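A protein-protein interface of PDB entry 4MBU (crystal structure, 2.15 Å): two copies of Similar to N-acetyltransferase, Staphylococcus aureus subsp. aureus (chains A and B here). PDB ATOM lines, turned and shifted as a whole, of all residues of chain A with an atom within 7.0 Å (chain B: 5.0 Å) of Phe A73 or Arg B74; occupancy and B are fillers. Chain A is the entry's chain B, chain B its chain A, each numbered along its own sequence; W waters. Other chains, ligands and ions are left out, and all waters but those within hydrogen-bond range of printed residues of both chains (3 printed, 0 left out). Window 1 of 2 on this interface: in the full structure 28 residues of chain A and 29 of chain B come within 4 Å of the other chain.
OE2 of Glu A84 is in salt-bridge range of NH2 of Arg B74 (2.7 Å).
The side-chain hydroxyl (OG1) of Thr A82 sits at hydrogen-bond distance from the backbone carbonyl oxygen (O) of Val B147, at 2.6 Å.
The backbone carbonyl oxygen of Gly A71 is in hydrogen-bond range of the backbone NH of Glu A84, at 2.9 Å.
The backbone carbonyl oxygen (O) of Arg B74 sits at hydrogen-bond distance from the side-chain hydroxyl (OG) of Ser B72, at 3.4 Å.
The guanidinium group (NE) of Arg B74 lies within hydrogen-bond range of the side-chain hydroxyl (OH) of Tyr B79, at 2.9 Å.
The guanidinium group (NE) of Arg A74 lies within hydrogen-bond range of the side-chain hydroxyl (OH) of Tyr A79 (2.9 Å).
The backbone carbonyl oxygen of Leu A157 is in hydrogen-bond range of the backbone NH of Leu A144, 2.9 Å away.
Tyr A31 touches Trp B76.
Tyr B79 touches Tyr A31.
Phe A73 touches Arg B74.
Phe A73 touches Leu B144.
Tyr A79 touches Val B147 (CA to O, 3.6 Å).
Leu A144 touches Phe B73.
Tyr B79 touches Val A147.
Leu A157 touches Arg B74.
OH of Tyr B79 touches CD2 of Leu A157, at 3.6 Å.
Phe A159 touches Phe B159.
Of chain B, only Arg B74 (3.98 Å) and Leu B144 (3.3 Å) come within 4 Å of Phe A73.
Ala A120 touches none of the printed residues of chain B.
Of the printed residues of chain B, Leu A157 touches Arg B74 and Tyr B79.
Printed residues of chain B within 4 Å of Phe A159: Phe B159 (3.4 Å).
Arg B74 touches just these residues of chain A: Phe A73, Glu A84 and Leu A157.
Of the printed residues of chain A, Trp B76 touches Tyr A31.
The nearest residue of chain B that does not touch Phe A73 is Val B147 (4.4 Å).
The nearest residue of chain A that does not touch Arg B74 is Phe A159 (4.1 Å).
Printed residues of chain A that touch a printed residue of chain B: Tyr A31, Phe A73, Tyr A79, Thr A82, Glu A84, Leu A144, Val A147, Leu A157 and Phe A159.
Hydrophobic or aromatic side chains of chain A that line the printed part of chain B: Tyr A31, Phe A73, Tyr A79, Leu A144, Leu A157 and Phe A159.
Among the printed residues, 12 pairs touch across the chains.
Among the printed residues, Asp or Glu carboxylates within 4 Å of a Lys or Arg side-chain nitrogen of the other chain: Glu A84 with Arg B74 (2.7 Å).
Phe A73 touches Arg B74, but with the chains exchanged Arg A74 does not touch Phe B73 (4.01 Å).
Phe A73 touches Leu B144, and with the chains exchanged Leu A144 touches Phe B73.
Tyr A79 touches Val B147, and with the chains exchanged Val A147 touches Tyr B79.
Phe B159 touches its own counterpart, Phe A159.
Water W2 lies within hydrogen-bond range of NH1 of Arg A74 (2.5 Å) and O of Phe B73 (3.3 Å).
Water W1 lies within hydrogen-bond range of NH1 of Arg B74 and O of Phe A73.
Water W3 bridges the side-chain hydroxyl of Thr A82 and the backbone carbonyl oxygen of Val B147.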
ATOM      1  N   TYR A  31     -26.883  28.857  26.024  1.00  0.00           N
ATOM      2  CA  TYR A  31     -27.073  28.539  27.447  1.00  0.00           C
ATOM      3  C   TYR A  31     -27.382  29.788  28.302  1.00  0.00           C
ATOM      4  O   TYR A  31     -26.724  30.055  29.312  1.00  0.00           O
ATOM      5  CB  TYR A  31     -25.865  27.777  28.012  1.00  0.00           C
ATOM      6  CG  TYR A  31     -25.784  26.304  27.631  1.00  0.00           C
ATOM      7  CD1 TYR A  31     -26.413  25.821  26.498  1.00  0.00           C
ATOM      8  CD2 TYR A  31     -25.100  25.398  28.432  1.00  0.00           C
ATOM      9  CE1 TYR A  31     -26.339  24.476  26.155  1.00  0.00           C
ATOM     10  CE2 TYR A  31     -25.016  24.059  28.096  1.00  0.00           C
ATOM     11  CZ  TYR A  31     -25.634  23.603  26.956  1.00  0.00           C
ATOM     12  OH  TYR A  31     -25.563  22.265  26.613  1.00  0.00           O
ATOM     13  N   GLY A  71     -14.059  33.417  18.642  1.00  0.00           N
ATOM     14  CA  GLY A  71     -13.333  34.148  19.667  1.00  0.00           C
ATOM     15  C   GLY A  71     -12.594  33.194  20.584  1.00  0.00           C
ATOM     16  O   GLY A  71     -12.351  32.043  20.221  1.00  0.00           O
ATOM     17  N   SER A  72     -12.237  33.661  21.773  1.00  0.00           N
ATOM     18  CA  SER A  72     -11.470  32.830  22.699  1.00  0.00           C
ATOM     19  C   SER A  72     -12.236  31.570  23.111  1.00  0.00           C
ATOM     20  O   SER A  72     -13.457  31.599  23.260  1.00  0.00           O
ATOM     21  CB  SER A  72     -11.088  33.629  23.948  1.00  0.00           C
ATOM     22  OG  SER A  72     -10.353  32.819  24.848  1.00  0.00           O
ATOM     23  N   PHE A  73     -11.520  30.462  23.286  1.00  0.00           N
ATOM     24  CA  PHE A  73     -12.134  29.248  23.809  1.00  0.00           C
ATOM     25  C   PHE A  73     -12.035  29.188  25.346  1.00  0.00           C
ATOM     26  O   PHE A  73     -13.036  28.983  26.038  1.00  0.00           O
ATOM     27  CB  PHE A  73     -11.488  28.010  23.174  1.00  0.00           C
ATOM     28  CG  PHE A  73     -11.820  26.722  23.878  1.00  0.00           C
ATOM     29  CD1 PHE A  73     -13.134  26.342  24.094  1.00  0.00           C
ATOM     30  CD2 PHE A  73     -10.809  25.881  24.302  1.00  0.00           C
ATOM     31  CE1 PHE A  73     -13.427  25.145  24.739  1.00  0.00           C
ATOM     32  CE2 PHE A  73     -11.096  24.693  24.939  1.00  0.00           C
ATOM     33  CZ  PHE A  73     -12.404  24.330  25.163  1.00  0.00           C
ATOM     34  N   ARG A  74     -10.815  29.321  25.867  1.00  0.00           N
ATOM     35  CA  ARG A  74     -10.590  29.433  27.307  1.00  0.00           C
ATOM     36  C   ARG A  74      -9.617  30.583  27.503  1.00  0.00           C
ATOM     37  O   ARG A  74      -8.819  30.854  26.616  1.00  0.00           O
ATOM     38  CB  ARG A  74     -10.053  28.114  27.897  1.00  0.00           C
ATOM     39  CG  ARG A  74     -11.145  27.069  28.152  1.00  0.00           C
ATOM     40  CD  ARG A  74     -10.611  25.631  28.301  1.00  0.00           C
ATOM     41  NE  ARG A  74      -9.913  25.395  29.573  1.00  0.00           N
ATOM     42  CZ  ARG A  74     -10.521  25.174  30.738  1.00  0.00           C
ATOM     43  NH1 ARG A  74     -11.847  25.182  30.808  1.00  0.00           N
ATOM     44  NH2 ARG A  74      -9.802  24.957  31.838  1.00  0.00           N
ATOM     45  N   PRO A  75      -9.709  31.288  28.646  1.00  0.00           N
ATOM     46  CA  PRO A  75      -8.948  32.528  28.875  1.00  0.00           C
ATOM     47  C   PRO A  75      -7.635  32.324  29.640  1.00  0.00           C
ATOM     48  O   PRO A  75      -7.521  32.651  30.829  1.00  0.00           O
ATOM     49  CB  PRO A  75      -9.912  33.368  29.719  1.00  0.00           C
ATOM     50  CG  PRO A  75     -10.651  32.336  30.531  1.00  0.00           C
ATOM     51  CD  PRO A  75     -10.739  31.077  29.682  1.00  0.00           C
ATOM     52  N   TRP A  76      -6.648  31.775  28.947  1.00  0.00           N
ATOM     53  CA  TRP A  76      -5.291  31.657  29.463  1.00  0.00           C
ATOM     54  C   TRP A  76      -4.419  31.777  28.219  1.00  0.00           C
ATOM     55  O   TRP A  76      -4.805  31.286  27.150  1.00  0.00           O
ATOM     56  CB  TRP A  76      -5.066  30.298  30.152  1.00  0.00           C
ATOM     57  CG  TRP A  76      -5.618  30.179  31.558  1.00  0.00           C
ATOM     58  CD1 TRP A  76      -4.975  30.508  32.716  1.00  0.00           C
ATOM     59  CD2 TRP A  76      -6.909  29.672  31.947  1.00  0.00           C
ATOM     60  NE1 TRP A  76      -5.786  30.253  33.796  1.00  0.00           N
ATOM     61  CE2 TRP A  76      -6.979  29.743  33.352  1.00  0.00           C
ATOM     62  CE3 TRP A  76      -8.013  29.181  31.242  1.00  0.00           C
ATOM     63  CZ2 TRP A  76      -8.113  29.336  34.071  1.00  0.00           C
ATOM     64  CZ3 TRP A  76      -9.138  28.774  31.955  1.00  0.00           C
ATOM     65  CH2 TRP A  76      -9.178  28.854  33.354  1.00  0.00           C
ATOM     66  N   TYR A  79      -3.678  29.184  25.308  1.00  0.00           N
ATOM     67  CA  TYR A  79      -4.778  28.787  24.410  1.00  0.00           C
ATOM     68  C   TYR A  79      -4.795  29.673  23.175  1.00  0.00           C
ATOM     69  O   TYR A  79      -5.786  29.714  22.440  1.00  0.00           O
ATOM     70  CB  TYR A  79      -6.133  28.891  25.111  1.00  0.00           C
ATOM     71  CG  TYR A  79      -6.376  27.840  26.163  1.00  0.00           C
ATOM     72  CD1 TYR A  79      -6.081  28.083  27.499  1.00  0.00           C
ATOM     73  CD2 TYR A  79      -6.903  26.601  25.819  1.00  0.00           C
ATOM     74  CE1 TYR A  79      -6.312  27.117  28.466  1.00  0.00           C
ATOM     75  CE2 TYR A  79      -7.126  25.629  26.772  1.00  0.00           C
ATOM     76  CZ  TYR A  79      -6.837  25.894  28.090  1.00  0.00           C
ATOM     77  OH  TYR A  79      -7.066  24.922  29.035  1.00  0.00           O
ATOM     78  N   THR A  82      -6.131  28.559  19.691  1.00  0.00           N
ATOM     79  CA  THR A  82      -7.443  27.893  19.709  1.00  0.00           C
ATOM     80  C   THR A  82      -8.547  28.944  19.718  1.00  0.00           C
ATOM     81  O   THR A  82      -8.486  29.907  20.498  1.00  0.00           O
ATOM     82  CB  THR A  82      -7.597  27.053  20.981  1.00  0.00           C
ATOM     83  OG1 THR A  82      -6.533  26.101  21.049  1.00  0.00           O
ATOM     84  CG2 THR A  82      -8.940  26.318  21.009  1.00  0.00           C
ATOM     85  N   ILE A  83      -9.553  28.764  18.862  1.00  0.00           N
ATOM     86  CA  ILE A  83     -10.734  29.634  18.865  1.00  0.00           C
ATOM     87  C   ILE A  83     -12.009  28.810  18.927  1.00  0.00           C
ATOM     88  O   ILE A  83     -12.049  27.679  18.455  1.00  0.00           O
ATOM     89  CB  ILE A  83     -10.795  30.526  17.604  1.00  0.00           C
ATOM     90  CG1 ILE A  83     -10.470  29.697  16.370  1.00  0.00           C
ATOM     91  CG2 ILE A  83      -9.835  31.722  17.727  1.00  0.00           C
ATOM     92  CD1 ILE A  83     -10.665  30.434  15.067  1.00  0.00           C
ATOM     93  N   GLU A  84     -13.062  29.375  19.503  1.00  0.00           N
ATOM     94  CA  GLU A  84     -14.359  28.716  19.487  1.00  0.00           C
ATOM     95  C   GLU A  84     -15.292  29.518  18.612  1.00  0.00           C
ATOM     96  O   GLU A  84     -15.358  30.752  18.728  1.00  0.00           O
ATOM     97  CB  GLU A  84     -14.935  28.595  20.900  1.00  0.00           C
ATOM     98  CG  GLU A  84     -16.342  27.990  20.938  1.00  0.00           C
ATOM     99  CD  GLU A  84     -16.836  27.708  22.357  1.00  0.00           C
ATOM    100  OE1 GLU A  84     -16.037  27.820  23.317  1.00  0.00           O
ATOM    101  OE2 GLU A  84     -18.034  27.374  22.514  1.00  0.00           O
ATOM    102  N   THR A 117      -6.467  25.351  16.027  1.00  0.00           N
ATOM    103  CA  THR A 117      -7.595  24.517  16.432  1.00  0.00           C
ATOM    104  C   THR A 117      -8.907  25.305  16.520  1.00  0.00           C
ATOM    105  O   THR A 117      -8.993  26.344  17.211  1.00  0.00           O
ATOM    106  CB  THR A 117      -7.292  23.809  17.772  1.00  0.00           C
ATOM    107  OG1 THR A 117      -6.069  23.075  17.642  1.00  0.00           O
ATOM    108  CG2 THR A 117      -8.417  22.844  18.158  1.00  0.00           C
ATOM    109  N   VAL A 119     -12.854  25.102  17.632  1.00  0.00           N
ATOM    110  CA  VAL A 119     -13.705  24.332  18.541  1.00  0.00           C
ATOM    111  C   VAL A 119     -15.174  24.780  18.482  1.00  0.00           C
ATOM    112  O   VAL A 119     -15.478  25.978  18.409  1.00  0.00           O
ATOM    113  CB  VAL A 119     -13.209  24.448  20.009  1.00  0.00           C
ATOM    114  CG1 VAL A 119     -14.043  23.581  20.923  1.00  0.00           C
ATOM    115  CG2 VAL A 119     -11.746  24.053  20.121  1.00  0.00           C
ATOM    116  N   ALA A 120     -16.075  23.800  18.497  1.00  0.00           N
ATOM    117  CA  ALA A 120     -17.511  24.041  18.587  1.00  0.00           C
ATOM    118  C   ALA A 120     -18.054  23.377  19.832  1.00  0.00           C
ATOM    119  O   ALA A 120     -17.805  22.194  20.078  1.00  0.00           O
ATOM    120  CB  ALA A 120     -18.231  23.484  17.366  1.00  0.00           C
ATOM    121  N   GLY A 121     -18.794  24.139  20.628  1.00  0.00           N
ATOM    122  CA  GLY A 121     -19.561  23.560  21.712  1.00  0.00           C
ATOM    123  C   GLY A 121     -20.955  23.352  21.157  1.00  0.00           C
ATOM    124  O   GLY A 121     -21.647  24.306  20.866  1.00  0.00           O
ATOM    125  N   ILE A 122     -21.377  22.109  20.971  1.00  0.00           N
ATOM    126  CA  ILE A 122     -22.681  21.870  20.372  1.00  0.00           C
ATOM    127  C   ILE A 122     -23.559  21.100  21.348  1.00  0.00           C
ATOM    128  O   ILE A 122     -23.129  20.083  21.890  1.00  0.00           O
ATOM    129  CB  ILE A 122     -22.559  21.052  19.068  1.00  0.00           C
ATOM    130  CG1 ILE A 122     -21.516  21.660  18.130  1.00  0.00           C
ATOM    131  CG2 ILE A 122     -23.906  20.985  18.359  1.00  0.00           C
ATOM    132  CD1 ILE A 122     -21.299  20.837  16.868  1.00  0.00           C
ATOM    133  N   LEU A 144     -19.536  16.555  27.718  1.00  0.00           N
ATOM    134  CA  LEU A 144     -19.703  16.817  29.135  1.00  0.00           C
ATOM    135  C   LEU A 144     -21.183  16.698  29.439  1.00  0.00           C
ATOM    136  O   LEU A 144     -22.004  17.407  28.858  1.00  0.00           O
ATOM    137  CB  LEU A 144     -19.196  18.210  29.477  1.00  0.00           C
ATOM    138  CG  LEU A 144     -17.678  18.368  29.492  1.00  0.00           C
ATOM    139  CD1 LEU A 144     -17.294  19.828  29.458  1.00  0.00           C
ATOM    140  CD2 LEU A 144     -17.115  17.737  30.736  1.00  0.00           C
ATOM    141  N   VAL A 147     -23.967  19.495  32.072  1.00  0.00           N
ATOM    142  CA  VAL A 147     -23.229  20.734  32.304  1.00  0.00           C
ATOM    143  C   VAL A 147     -24.147  21.926  32.239  1.00  0.00           C
ATOM    144  O   VAL A 147     -23.811  22.990  32.764  1.00  0.00           O
ATOM    145  CB  VAL A 147     -22.086  20.989  31.288  1.00  0.00           C
ATOM    146  CG1 VAL A 147     -20.827  20.269  31.700  1.00  0.00           C
ATOM    147  CG2 VAL A 147     -22.532  20.644  29.876  1.00  0.00           C
ATOM    148  N   LEU A 157     -23.174  18.878  26.703  1.00  0.00           N
ATOM    149  CA  LEU A 157     -22.468  19.666  25.706  1.00  0.00           C
ATOM    150  C   LEU A 157     -21.417  18.806  25.032  1.00  0.00           C
ATOM    151  O   LEU A 157     -20.516  18.295  25.679  1.00  0.00           O
ATOM    152  CB  LEU A 157     -21.793  20.871  26.358  1.00  0.00           C
ATOM    153  CG  LEU A 157     -21.095  21.829  25.391  1.00  0.00           C
ATOM    154  CD1 LEU A 157     -22.119  22.711  24.680  1.00  0.00           C
ATOM    155  CD2 LEU A 157     -20.063  22.674  26.130  1.00  0.00           C
ATOM    156  N   PHE A 159     -18.261  18.493  22.472  1.00  0.00           N
ATOM    157  CA  PHE A 159     -17.220  19.344  21.915  1.00  0.00           C
ATOM    158  C   PHE A 159     -16.796  18.730  20.596  1.00  0.00           C
ATOM    159  O   PHE A 159     -16.547  17.530  20.530  1.00  0.00           O
ATOM    160  CB  PHE A 159     -16.027  19.427  22.869  1.00  0.00           C
ATOM    161  CG  PHE A 159     -16.121  20.549  23.870  1.00  0.00           C
ATOM    162  CD1 PHE A 159     -15.890  20.311  25.219  1.00  0.00           C
ATOM    163  CD2 PHE A 159     -16.406  21.842  23.460  1.00  0.00           C
ATOM    164  CE1 PHE A 159     -15.963  21.346  26.149  1.00  0.00           C
ATOM    165  CE2 PHE A 159     -16.484  22.884  24.387  1.00  0.00           C
ATOM    166  CZ  PHE A 159     -16.261  22.636  25.731  1.00  0.00           C
ATOM    167  N   SER B  72     -16.407  29.270  38.075  1.00  0.00           N
ATOM    168  CA  SER B  72     -17.227  29.069  36.882  1.00  0.00           C
ATOM    169  C   SER B  72     -16.513  28.186  35.860  1.00  0.00           C
ATOM    170  O   SER B  72     -15.300  28.277  35.709  1.00  0.00           O
ATOM    171  CB  SER B  72     -17.575  30.425  36.259  1.00  0.00           C
ATOM    172  OG  SER B  72     -17.976  30.293  34.911  1.00  0.00           O
ATOM    173  N   PHE B  73     -17.263  27.325  35.172  1.00  0.00           N
ATOM    174  CA  PHE B  73     -16.678  26.509  34.110  1.00  0.00           C
ATOM    175  C   PHE B  73     -16.759  27.234  32.760  1.00  0.00           C
ATOM    176  O   PHE B  73     -15.738  27.448  32.103  1.00  0.00           O
ATOM    177  CB  PHE B  73     -17.341  25.131  34.039  1.00  0.00           C
ATOM    178  CG  PHE B  73     -17.031  24.380  32.771  1.00  0.00           C
ATOM    179  CD1 PHE B  73     -15.714  24.108  32.408  1.00  0.00           C
ATOM    180  CD2 PHE B  73     -18.054  23.947  31.943  1.00  0.00           C
ATOM    181  CE1 PHE B  73     -15.430  23.426  31.228  1.00  0.00           C
ATOM    182  CE2 PHE B  73     -17.785  23.259  30.774  1.00  0.00           C
ATOM    183  CZ  PHE B  73     -16.467  22.999  30.414  1.00  0.00           C
ATOM    184  N   ARG B  74     -17.973  27.604  32.344  1.00  0.00           N
ATOM    185  CA  ARG B  74     -18.157  28.433  31.152  1.00  0.00           C
ATOM    186  C   ARG B  74     -19.095  29.569  31.512  1.00  0.00           C
ATOM    187  O   ARG B  74     -20.019  29.377  32.302  1.00  0.00           O
ATOM    188  CB  ARG B  74     -18.707  27.619  29.972  1.00  0.00           C
ATOM    189  CG  ARG B  74     -17.615  26.901  29.180  1.00  0.00           C
ATOM    190  CD  ARG B  74     -18.139  25.735  28.341  1.00  0.00           C
ATOM    191  NE  ARG B  74     -18.844  26.151  27.125  1.00  0.00           N
ATOM    192  CZ  ARG B  74     -18.241  26.552  26.007  1.00  0.00           C
ATOM    193  NH1 ARG B  74     -16.915  26.628  25.953  1.00  0.00           N
ATOM    194  NH2 ARG B  74     -18.967  26.899  24.950  1.00  0.00           N
ATOM    195  N   PRO B  75     -18.849  30.767  30.950  1.00  0.00           N
ATOM    196  CA  PRO B  75     -19.581  31.976  31.354  1.00  0.00           C
ATOM    197  C   PRO B  75     -20.893  32.152  30.597  1.00  0.00           C
ATOM    198  O   PRO B  75     -20.957  32.919  29.632  1.00  0.00           O
ATOM    199  CB  PRO B  75     -18.613  33.111  30.989  1.00  0.00           C
ATOM    200  CG  PRO B  75     -17.851  32.575  29.805  1.00  0.00           C
ATOM    201  CD  PRO B  75     -17.779  31.062  29.973  1.00  0.00           C
ATOM    202  N   TRP B  76     -21.924  31.440  31.038  1.00  0.00           N
ATOM    203  CA  TRP B  76     -23.281  31.605  30.528  1.00  0.00           C
ATOM    204  C   TRP B  76     -24.163  31.104  31.663  1.00  0.00           C
ATOM    205  O   TRP B  76     -23.829  30.104  32.289  1.00  0.00           O
ATOM    206  CB  TRP B  76     -23.523  30.769  29.257  1.00  0.00           C
ATOM    207  CG  TRP B  76     -22.986  31.357  27.969  1.00  0.00           C
ATOM    208  CD1 TRP B  76     -23.618  32.255  27.147  1.00  0.00           C
ATOM    209  CD2 TRP B  76     -21.722  31.069  27.346  1.00  0.00           C
ATOM    210  NE1 TRP B  76     -22.821  32.544  26.062  1.00  0.00           N
ATOM    211  CE2 TRP B  76     -21.654  31.833  26.160  1.00  0.00           C
ATOM    212  CE3 TRP B  76     -20.639  30.245  27.679  1.00  0.00           C
ATOM    213  CZ2 TRP B  76     -20.542  31.799  25.308  1.00  0.00           C
ATOM    214  CZ3 TRP B  76     -19.535  30.213  26.827  1.00  0.00           C
ATOM    215  CH2 TRP B  76     -19.497  30.985  25.658  1.00  0.00           C
ATOM    216  N   TYR B  79     -24.955  27.379  32.797  1.00  0.00           N
ATOM    217  CA  TYR B  79     -23.892  26.539  33.373  1.00  0.00           C
ATOM    218  C   TYR B  79     -23.830  26.691  34.887  1.00  0.00           C
ATOM    219  O   TYR B  79     -22.837  26.300  35.516  1.00  0.00           O
ATOM    220  CB  TYR B  79     -22.523  26.929  32.807  1.00  0.00           C
ATOM    221  CG  TYR B  79     -22.300  26.573  31.356  1.00  0.00           C
ATOM    222  CD1 TYR B  79     -22.546  27.496  30.351  1.00  0.00           C
ATOM    223  CD2 TYR B  79     -21.825  25.318  30.998  1.00  0.00           C
ATOM    224  CE1 TYR B  79     -22.326  27.177  29.017  1.00  0.00           C
ATOM    225  CE2 TYR B  79     -21.607  24.985  29.677  1.00  0.00           C
ATOM    226  CZ  TYR B  79     -21.860  25.921  28.695  1.00  0.00           C
ATOM    227  OH  TYR B  79     -21.646  25.591  27.392  1.00  0.00           O
ATOM    228  N   LEU B 144      -9.476  17.530  24.171  1.00  0.00           N
ATOM    229  CA  LEU B 144      -9.306  18.484  23.085  1.00  0.00           C
ATOM    230  C   LEU B 144      -7.831  18.522  22.728  1.00  0.00           C
ATOM    231  O   LEU B 144      -6.990  18.892  23.549  1.00  0.00           O
ATOM    232  CB  LEU B 144      -9.808  19.858  23.496  1.00  0.00           C
ATOM    233  CG  LEU B 144     -11.320  19.979  23.666  1.00  0.00           C
ATOM    234  CD1 LEU B 144     -11.622  21.137  24.546  1.00  0.00           C
ATOM    235  CD2 LEU B 144     -11.963  20.204  22.327  1.00  0.00           C
ATOM    236  N   VAL B 147      -4.956  22.130  21.845  1.00  0.00           N
ATOM    237  CA  VAL B 147      -5.631  23.359  22.267  1.00  0.00           C
ATOM    238  C   VAL B 147      -4.663  24.303  22.927  1.00  0.00           C
ATOM    239  O   VAL B 147      -4.933  25.510  23.008  1.00  0.00           O
ATOM    240  CB  VAL B 147      -6.797  23.140  23.275  1.00  0.00           C
ATOM    241  CG1 VAL B 147      -8.008  22.597  22.585  1.00  0.00           C
ATOM    242  CG2 VAL B 147      -6.350  22.242  24.431  1.00  0.00           C
ATOM    243  N   PHE B 159     -10.818  16.578  29.800  1.00  0.00           N
ATOM    244  CA  PHE B 159     -11.840  16.985  30.753  1.00  0.00           C
ATOM    245  C   PHE B 159     -12.261  15.771  31.563  1.00  0.00           C
ATOM    246  O   PHE B 159     -12.581  14.721  31.001  1.00  0.00           O
ATOM    247  CB  PHE B 159     -13.055  17.544  30.021  1.00  0.00           C
ATOM    248  CG  PHE B 159     -12.898  18.964  29.567  1.00  0.00           C
ATOM    249  CD1 PHE B 159     -13.264  19.329  28.286  1.00  0.00           C
ATOM    250  CD2 PHE B 159     -12.426  19.939  30.424  1.00  0.00           C
ATOM    251  CE1 PHE B 159     -13.141  20.633  27.858  1.00  0.00           C
ATOM    252  CE2 PHE B 159     -12.295  21.254  29.995  1.00  0.00           C
ATOM    253  CZ  PHE B 159     -12.657  21.597  28.714  1.00  0.00           C
HETATM  254  O   HOH W   1     -14.778  27.294  27.508  1.00  0.00           O
HETATM  255  O   HOH W   2     -13.851  26.181  29.775  1.00  0.00           O
HETATM  256  O   HOH W   3      -4.053  25.854  19.875  1.00  0.00           O
